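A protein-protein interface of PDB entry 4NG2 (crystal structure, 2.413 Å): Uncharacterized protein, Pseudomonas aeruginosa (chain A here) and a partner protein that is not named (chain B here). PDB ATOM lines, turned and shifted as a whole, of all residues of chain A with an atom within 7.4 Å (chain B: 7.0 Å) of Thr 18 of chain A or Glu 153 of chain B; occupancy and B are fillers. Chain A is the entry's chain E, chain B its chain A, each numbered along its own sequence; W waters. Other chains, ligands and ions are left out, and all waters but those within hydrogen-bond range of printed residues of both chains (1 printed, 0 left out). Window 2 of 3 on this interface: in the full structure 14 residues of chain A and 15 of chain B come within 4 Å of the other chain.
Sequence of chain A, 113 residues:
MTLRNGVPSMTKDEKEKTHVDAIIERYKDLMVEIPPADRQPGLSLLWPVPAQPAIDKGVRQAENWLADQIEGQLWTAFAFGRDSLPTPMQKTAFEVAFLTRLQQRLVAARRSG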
ATOM      1  N   LYS A  17      19.255 -22.472   0.388  1.00  0.00           N
ATOM      2  CA  LYS A  17      19.923 -23.080   1.537  1.00  0.00           C
ATOM      3  C   LYS A  17      20.593 -22.011   2.401  1.00  0.00           C
ATOM      4  O   LYS A  17      21.706 -21.599   2.124  1.00  0.00           O
ATOM      5  CB  LYS A  17      20.959 -24.104   1.062  1.00  0.00           C
ATOM      6  CG  LYS A  17      21.204 -25.237   2.042  1.00  0.00           C
ATOM      7  CD  LYS A  17      19.885 -25.698   2.637  1.00  0.00           C
ATOM      8  CE  LYS A  17      20.042 -27.021   3.341  1.00  0.00           C
ATOM      9  NZ  LYS A  17      20.564 -28.056   2.404  1.00  0.00           N
ATOM     10  N   THR A  18      19.908 -21.552   3.441  1.00  0.00           N
ATOM     11  CA  THR A  18      20.473 -20.534   4.326  1.00  0.00           C
ATOM     12  C   THR A  18      21.743 -21.054   4.999  1.00  0.00           C
ATOM     13  O   THR A  18      22.025 -22.252   4.933  1.00  0.00           O
ATOM     14  CB  THR A  18      19.480 -20.147   5.431  1.00  0.00           C
ATOM     15  OG1 THR A  18      18.139 -20.303   4.950  1.00  0.00           O
ATOM     16  CG2 THR A  18      19.710 -18.719   5.861  1.00  0.00           C
ATOM     17  N   HIS A  19      22.506 -20.169   5.645  1.00  0.00           N
ATOM     18  CA  HIS A  19      23.663 -20.619   6.425  1.00  0.00           C
ATOM     19  C   HIS A  19      23.208 -21.490   7.592  1.00  0.00           C
ATOM     20  O   HIS A  19      23.607 -22.664   7.708  1.00  0.00           O
ATOM     21  CB  HIS A  19      24.500 -19.454   6.965  1.00  0.00           C
ATOM     22  CG  HIS A  19      25.556 -19.882   7.944  1.00  0.00           C
ATOM     23  ND1 HIS A  19      26.374 -20.971   7.726  1.00  0.00           N
ATOM     24  CD2 HIS A  19      25.912 -19.383   9.152  1.00  0.00           C
ATOM     25  CE1 HIS A  19      27.196 -21.116   8.751  1.00  0.00           C
ATOM     26  NE2 HIS A  19      26.934 -20.165   9.631  1.00  0.00           N
ATOM     27  N   VAL A  20      22.366 -20.912   8.451  1.00  0.00           N
ATOM     28  CA  VAL A  20      21.880 -21.617   9.627  1.00  0.00           C
ATOM     29  C   VAL A  20      21.150 -22.922   9.288  1.00  0.00           C
ATOM     30  O   VAL A  20      21.193 -23.861  10.074  1.00  0.00           O
ATOM     31  CB  VAL A  20      20.995 -20.728  10.514  1.00  0.00           C
ATOM     32  CG1 VAL A  20      21.722 -19.446  10.872  1.00  0.00           C
ATOM     33  CG2 VAL A  20      19.686 -20.439   9.827  1.00  0.00           C
ATOM     34  N   ASP A  21      20.497 -22.987   8.125  1.00  0.00           N
ATOM     35  CA  ASP A  21      19.827 -24.219   7.677  1.00  0.00           C
ATOM     36  C   ASP A  21      20.816 -25.243   7.150  1.00  0.00           C
ATOM     37  O   ASP A  21      20.555 -26.440   7.167  1.00  0.00           O
ATOM     38  CB  ASP A  21      18.790 -23.930   6.582  1.00  0.00           C
ATOM     39  CG  ASP A  21      17.594 -23.148   7.099  1.00  0.00           C
ATOM     40  OD1 ASP A  21      17.190 -23.386   8.258  1.00  0.00           O
ATOM     41  OD2 ASP A  21      17.061 -22.294   6.352  1.00  0.00           O
ATOM     42  N   ALA A  22      21.948 -24.762   6.660  1.00  0.00           N
ATOM     43  CA  ALA A  22      22.921 -25.634   6.036  1.00  0.00           C
ATOM     44  C   ALA A  22      23.685 -26.355   7.116  1.00  0.00           C
ATOM     45  O   ALA A  22      24.198 -27.448   6.887  1.00  0.00           O
ATOM     46  CB  ALA A  22      23.870 -24.837   5.170  1.00  0.00           C
ATOM     47  N   ILE A  23      23.775 -25.729   8.290  1.00  0.00           N
ATOM     48  CA  ILE A  23      24.389 -26.375   9.449  1.00  0.00           C
ATOM     49  C   ILE A  23      23.460 -27.468  10.002  1.00  0.00           C
ATOM     50  O   ILE A  23      23.914 -28.553  10.349  1.00  0.00           O
ATOM     51  CB  ILE A  23      24.744 -25.371  10.569  1.00  0.00           C
ATOM     52  CG1 ILE A  23      25.857 -24.405  10.111  1.00  0.00           C
ATOM     53  CG2 ILE A  23      25.173 -26.120  11.809  1.00  0.00           C
ATOM     54  CD1 ILE A  23      27.122 -25.095   9.606  1.00  0.00           C
ATOM     55  N   ILE A  24      22.162 -27.177  10.059  1.00  0.00           N
ATOM     56  CA  ILE A  24      21.163 -28.201  10.350  1.00  0.00           C
ATOM     57  C   ILE A  24      21.191 -29.392   9.373  1.00  0.00           C
ATOM     58  O   ILE A  24      21.099 -30.540   9.805  1.00  0.00           O
ATOM     59  CB  ILE A  24      19.748 -27.619  10.389  1.00  0.00           C
ATOM     60  CG1 ILE A  24      19.665 -26.446  11.376  1.00  0.00           C
ATOM     61  CG2 ILE A  24      18.751 -28.700  10.757  1.00  0.00           C
ATOM     62  CD1 ILE A  24      19.756 -26.838  12.825  1.00  0.00           C
ATOM     63  N   VAL B 146      27.555 -15.833  15.184  1.00  0.00           N
ATOM     64  CA  VAL B 146      27.055 -16.505  13.999  1.00  0.00           C
ATOM     65  C   VAL B 146      26.530 -15.489  12.992  1.00  0.00           C
ATOM     66  O   VAL B 146      25.848 -14.530  13.351  1.00  0.00           O
ATOM     67  CB  VAL B 146      25.925 -17.474  14.380  1.00  0.00           C
ATOM     68  CG1 VAL B 146      24.804 -16.718  15.072  1.00  0.00           C
ATOM     69  CG2 VAL B 146      25.413 -18.240  13.154  1.00  0.00           C
ATOM     70  N   GLU B 147      26.841 -15.717  11.725  1.00  0.00           N
ATOM     71  CA  GLU B 147      26.388 -14.843  10.658  1.00  0.00           C
ATOM     72  C   GLU B 147      25.069 -15.352  10.082  1.00  0.00           C
ATOM     73  O   GLU B 147      25.061 -16.221   9.216  1.00  0.00           O
ATOM     74  CB  GLU B 147      27.459 -14.779   9.566  1.00  0.00           C
ATOM     75  CG  GLU B 147      28.898 -14.870  10.112  1.00  0.00           C
ATOM     76  CD  GLU B 147      29.967 -14.817   9.022  1.00  0.00           C
ATOM     77  OE1 GLU B 147      29.606 -14.755   7.825  1.00  0.00           O
ATOM     78  OE2 GLU B 147      31.173 -14.830   9.365  1.00  0.00           O
ATOM     79  N   ALA B 148      23.953 -14.813  10.567  1.00  0.00           N
ATOM     80  CA  ALA B 148      22.629 -15.232  10.089  1.00  0.00           C
ATOM     81  C   ALA B 148      21.860 -14.099   9.395  1.00  0.00           C
ATOM     82  O   ALA B 148      22.161 -12.922   9.602  1.00  0.00           O
ATOM     83  CB  ALA B 148      21.800 -15.816  11.238  1.00  0.00           C
ATOM     84  N   GLU B 149      20.858 -14.460   8.591  1.00  0.00           N
ATOM     85  CA  GLU B 149      20.121 -13.484   7.779  1.00  0.00           C
ATOM     86  C   GLU B 149      19.490 -12.367   8.617  1.00  0.00           C
ATOM     87  O   GLU B 149      19.374 -11.225   8.166  1.00  0.00           O
ATOM     88  CB  GLU B 149      19.059 -14.180   6.912  1.00  0.00           C
ATOM     89  CG  GLU B 149      19.211 -13.947   5.401  1.00  0.00           C
ATOM     90  CD  GLU B 149      18.699 -12.582   4.941  1.00  0.00           C
ATOM     91  OE1 GLU B 149      17.914 -11.951   5.678  1.00  0.00           O
ATOM     92  OE2 GLU B 149      19.079 -12.137   3.835  1.00  0.00           O
ATOM     93  N   ASN B 150      19.094 -12.700   9.839  1.00  0.00           N
ATOM     94  CA  ASN B 150      18.504 -11.728  10.754  1.00  0.00           C
ATOM     95  C   ASN B 150      18.511 -12.266  12.178  1.00  0.00           C
ATOM     96  O   ASN B 150      19.059 -13.335  12.423  1.00  0.00           O
ATOM     97  CB  ASN B 150      17.079 -11.417  10.331  1.00  0.00           C
ATOM     98  CG  ASN B 150      16.248 -12.659  10.185  1.00  0.00           C
ATOM     99  OD1 ASN B 150      16.312 -13.350   9.163  1.00  0.00           O
ATOM    100  ND2 ASN B 150      15.468 -12.964  11.210  1.00  0.00           N
ATOM    101  N   ARG B 151      17.899 -11.544  13.115  1.00  0.00           N
ATOM    102  CA  ARG B 151      17.922 -11.967  14.513  1.00  0.00           C
ATOM    103  C   ARG B 151      17.019 -13.170  14.795  1.00  0.00           C
ATOM    104  O   ARG B 151      17.384 -14.065  15.560  1.00  0.00           O
ATOM    105  CB  ARG B 151      17.578 -10.813  15.454  1.00  0.00           C
ATOM    106  CG  ARG B 151      18.637 -10.582  16.512  1.00  0.00           C
ATOM    107  CD  ARG B 151      18.066  -9.960  17.773  1.00  0.00           C
ATOM    108  NE  ARG B 151      17.148  -8.854  17.500  1.00  0.00           N
ATOM    109  CZ  ARG B 151      17.498  -7.685  16.955  1.00  0.00           C
ATOM    110  NH1 ARG B 151      18.762  -7.454  16.595  1.00  0.00           N
ATOM    111  NH2 ARG B 151      16.576  -6.741  16.758  1.00  0.00           N
ATOM    112  N   ALA B 152      15.840 -13.195  14.184  1.00  0.00           N
ATOM    113  CA  ALA B 152      14.958 -14.345  14.350  1.00  0.00           C
ATOM    114  C   ALA B 152      15.696 -15.645  14.013  1.00  0.00           C
ATOM    115  O   ALA B 152      15.856 -16.500  14.869  1.00  0.00           O
ATOM    116  CB  ALA B 152      13.682 -14.200  13.510  1.00  0.00           C
ATOM    117  N   GLU B 153      16.145 -15.781  12.770  1.00  0.00           N
ATOM    118  CA  GLU B 153      16.909 -16.946  12.344  1.00  0.00           C
ATOM    119  C   GLU B 153      18.066 -17.267  13.305  1.00  0.00           C
ATOM    120  O   GLU B 153      18.279 -18.423  13.657  1.00  0.00           O
ATOM    121  CB  GLU B 153      17.456 -16.729  10.935  1.00  0.00           C
ATOM    122  CG  GLU B 153      17.075 -17.800   9.917  1.00  0.00           C
ATOM    123  CD  GLU B 153      17.733 -17.554   8.568  1.00  0.00           C
ATOM    124  OE1 GLU B 153      17.093 -16.922   7.695  1.00  0.00           O
ATOM    125  OE2 GLU B 153      18.900 -17.976   8.391  1.00  0.00           O
ATOM    126  N   ALA B 154      18.800 -16.243  13.734  1.00  0.00           N
ATOM    127  CA  ALA B 154      19.928 -16.435  14.641  1.00  0.00           C
ATOM    128  C   ALA B 154      19.528 -16.987  16.011  1.00  0.00           C
ATOM    129  O   ALA B 154      20.178 -17.896  16.509  1.00  0.00           O
ATOM    130  CB  ALA B 154      20.740 -15.144  14.801  1.00  0.00           C
ATOM    131  N   ASN B 155      18.490 -16.432  16.628  1.00  0.00           N
ATOM    132  CA  ASN B 155      18.081 -16.896  17.953  1.00  0.00           C
ATOM    133  C   ASN B 155      17.444 -18.294  17.901  1.00  0.00           C
ATOM    134  O   ASN B 155      17.584 -19.082  18.844  1.00  0.00           O
ATOM    135  CB  ASN B 155      17.133 -15.910  18.644  1.00  0.00           C
ATOM    136  CG  ASN B 155      17.795 -14.578  18.976  1.00  0.00           C
ATOM    137  OD1 ASN B 155      18.987 -14.503  19.309  1.00  0.00           O
ATOM    138  ND2 ASN B 155      17.006 -13.507  18.894  1.00  0.00           N
ATOM    139  N   ARG B 156      16.741 -18.593  16.805  1.00  0.00           N
ATOM    140  CA  ARG B 156      16.187 -19.929  16.609  1.00  0.00           C
ATOM    141  C   ARG B 156      17.338 -20.908  16.448  1.00  0.00           C
ATOM    142  O   ARG B 156      17.347 -21.979  17.058  1.00  0.00           O
ATOM    143  CB  ARG B 156      15.258 -20.010  15.388  1.00  0.00           C
ATOM    144  CG  ARG B 156      13.789 -19.715  15.683  1.00  0.00           C
ATOM    145  CD  ARG B 156      12.859 -20.185  14.541  1.00  0.00           C
ATOM    146  NE  ARG B 156      13.372 -19.870  13.204  1.00  0.00           N
ATOM    147  CZ  ARG B 156      13.142 -18.726  12.559  1.00  0.00           C
ATOM    148  NH1 ARG B 156      12.409 -17.782  13.133  1.00  0.00           N
ATOM    149  NH2 ARG B 156      13.648 -18.526  11.341  1.00  0.00           N
ATOM    150  N   PHE B 157      18.313 -20.528  15.627  1.00  0.00           N
ATOM    151  CA  PHE B 157      19.463 -21.379  15.400  1.00  0.00           C
ATOM    152  C   PHE B 157      20.220 -21.675  16.697  1.00  0.00           C
ATOM    153  O   PHE B 157      20.581 -22.822  16.960  1.00  0.00           O
ATOM    154  CB  PHE B 157      20.413 -20.755  14.401  1.00  0.00           C
ATOM    155  CG  PHE B 157      21.695 -21.515  14.249  1.00  0.00           C
ATOM    156  CD1 PHE B 157      21.741 -22.667  13.486  1.00  0.00           C
ATOM    157  CD2 PHE B 157      22.854 -21.083  14.876  1.00  0.00           C
ATOM    158  CE1 PHE B 157      22.921 -23.363  13.347  1.00  0.00           C
ATOM    159  CE2 PHE B 157      24.034 -21.784  14.732  1.00  0.00           C
ATOM    160  CZ  PHE B 157      24.067 -22.916  13.963  1.00  0.00           C
ATOM    161  N   MET B 158      20.448 -20.642  17.499  1.00  0.00           N
ATOM    162  CA  MET B 158      21.237 -20.769  18.711  1.00  0.00           C
ATOM    163  C   MET B 158      20.497 -21.526  19.789  1.00  0.00           C
ATOM    164  O   MET B 158      21.117 -22.042  20.707  1.00  0.00           O
ATOM    165  CB  MET B 158      21.670 -19.397  19.243  1.00  0.00           C
ATOM    166  CG  MET B 158      22.810 -18.750  18.464  1.00  0.00           C
ATOM    167  SD  MET B 158      23.436 -17.268  19.287  1.00  0.00           S
ATOM    168  CE  MET B 158      22.194 -16.063  18.805  1.00  0.00           C
ATOM    169  N   GLU B 159      19.179 -21.601  19.700  1.00  0.00           N
ATOM    170  CA  GLU B 159      18.443 -22.334  20.721  1.00  0.00           C
ATOM    171  C   GLU B 159      18.495 -23.840  20.444  1.00  0.00           C
ATOM    172  O   GLU B 159      18.466 -24.649  21.377  1.00  0.00           O
ATOM    173  CB  GLU B 159      17.004 -21.844  20.833  1.00  0.00           C
ATOM    174  CG  GLU B 159      16.430 -22.016  22.225  1.00  0.00           C
ATOM    175  CD  GLU B 159      17.063 -21.072  23.233  1.00  0.00           C
ATOM    176  OE1 GLU B 159      17.044 -19.850  22.980  1.00  0.00           O
ATOM    177  OE2 GLU B 159      17.578 -21.549  24.276  1.00  0.00           O
HETATM  178  O   HOH W   1      29.014 -17.945  10.822  1.00  0.00           O
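N of Glu 153 of chain B sits close to ND2 of Asn 150 of chain B. The side-chain hydroxyl of Thr 18 of chain A is in hydrogen-bond range of the side-chain carboxylate of Asp 21 of chain A, 2.7 Å away.
Among the printed residues, merely in contact across the chains: Thr 18 of chain A with Glu 153 of chain B, Val 20 of chain A with Glu 153 of chain B, His 19 of chain A with Glu 147 of chain B, Val 20 of chain A with Phe 157 of chain B, Val 20 of chain A with Ala 148 of chain B and Ile 23 of chain A with Phe 157 of chain B.
Of the printed residues of chain B, Thr 18 of chain A touches Glu 153. Glu 153 of chain B touches two residues of chain A. Ala 152 of chain B touches none of the printed residues of chain A. Of the printed residues of chain B, His 19 of chain A touches Glu 147 (3.3 Å). Of the printed residues of chain A, Glu 147 of chain B touches His 19 (3.3 Å). Of the printed residues of chain B, Ile 23 of chain A touches Phe 157 (3.9 Å). Of the printed residues of chain A, Ala 148 of chain B touches Val 20 (3.6 Å). Printed residues of chain B within 4 Å of Val 20 of chain A: Ala 148, Glu 153 and Phe 157. Lys 17 of chain A touches none of the printed residues of chain B. Glu 149 of chain B touches none of the printed residues of chain A. The nearest residue of chain B that does not touch Thr 18 of chain A is Glu 149 of chain B (4.7 Å).
Of the 8 printed residues of chain A, 4 touch a printed residue of chain B. Hydrophobic or aromatic side chains of chain A that line the printed part of chain B: His 19, Val 20 and Ile 23. Of the 14 printed residues of chain B, 4 touch a printed residue of chain A. Hydrophobic or aromatic side chains of chain B within 4 Å of the printed part of chain A: Ala 148 and Phe 157.
Water W1 bridges the backbone NH of Glu 147 of chain B (3.2 Å) and a ring nitrogen (NE2) of His 19 of chain A (3.3 Å).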
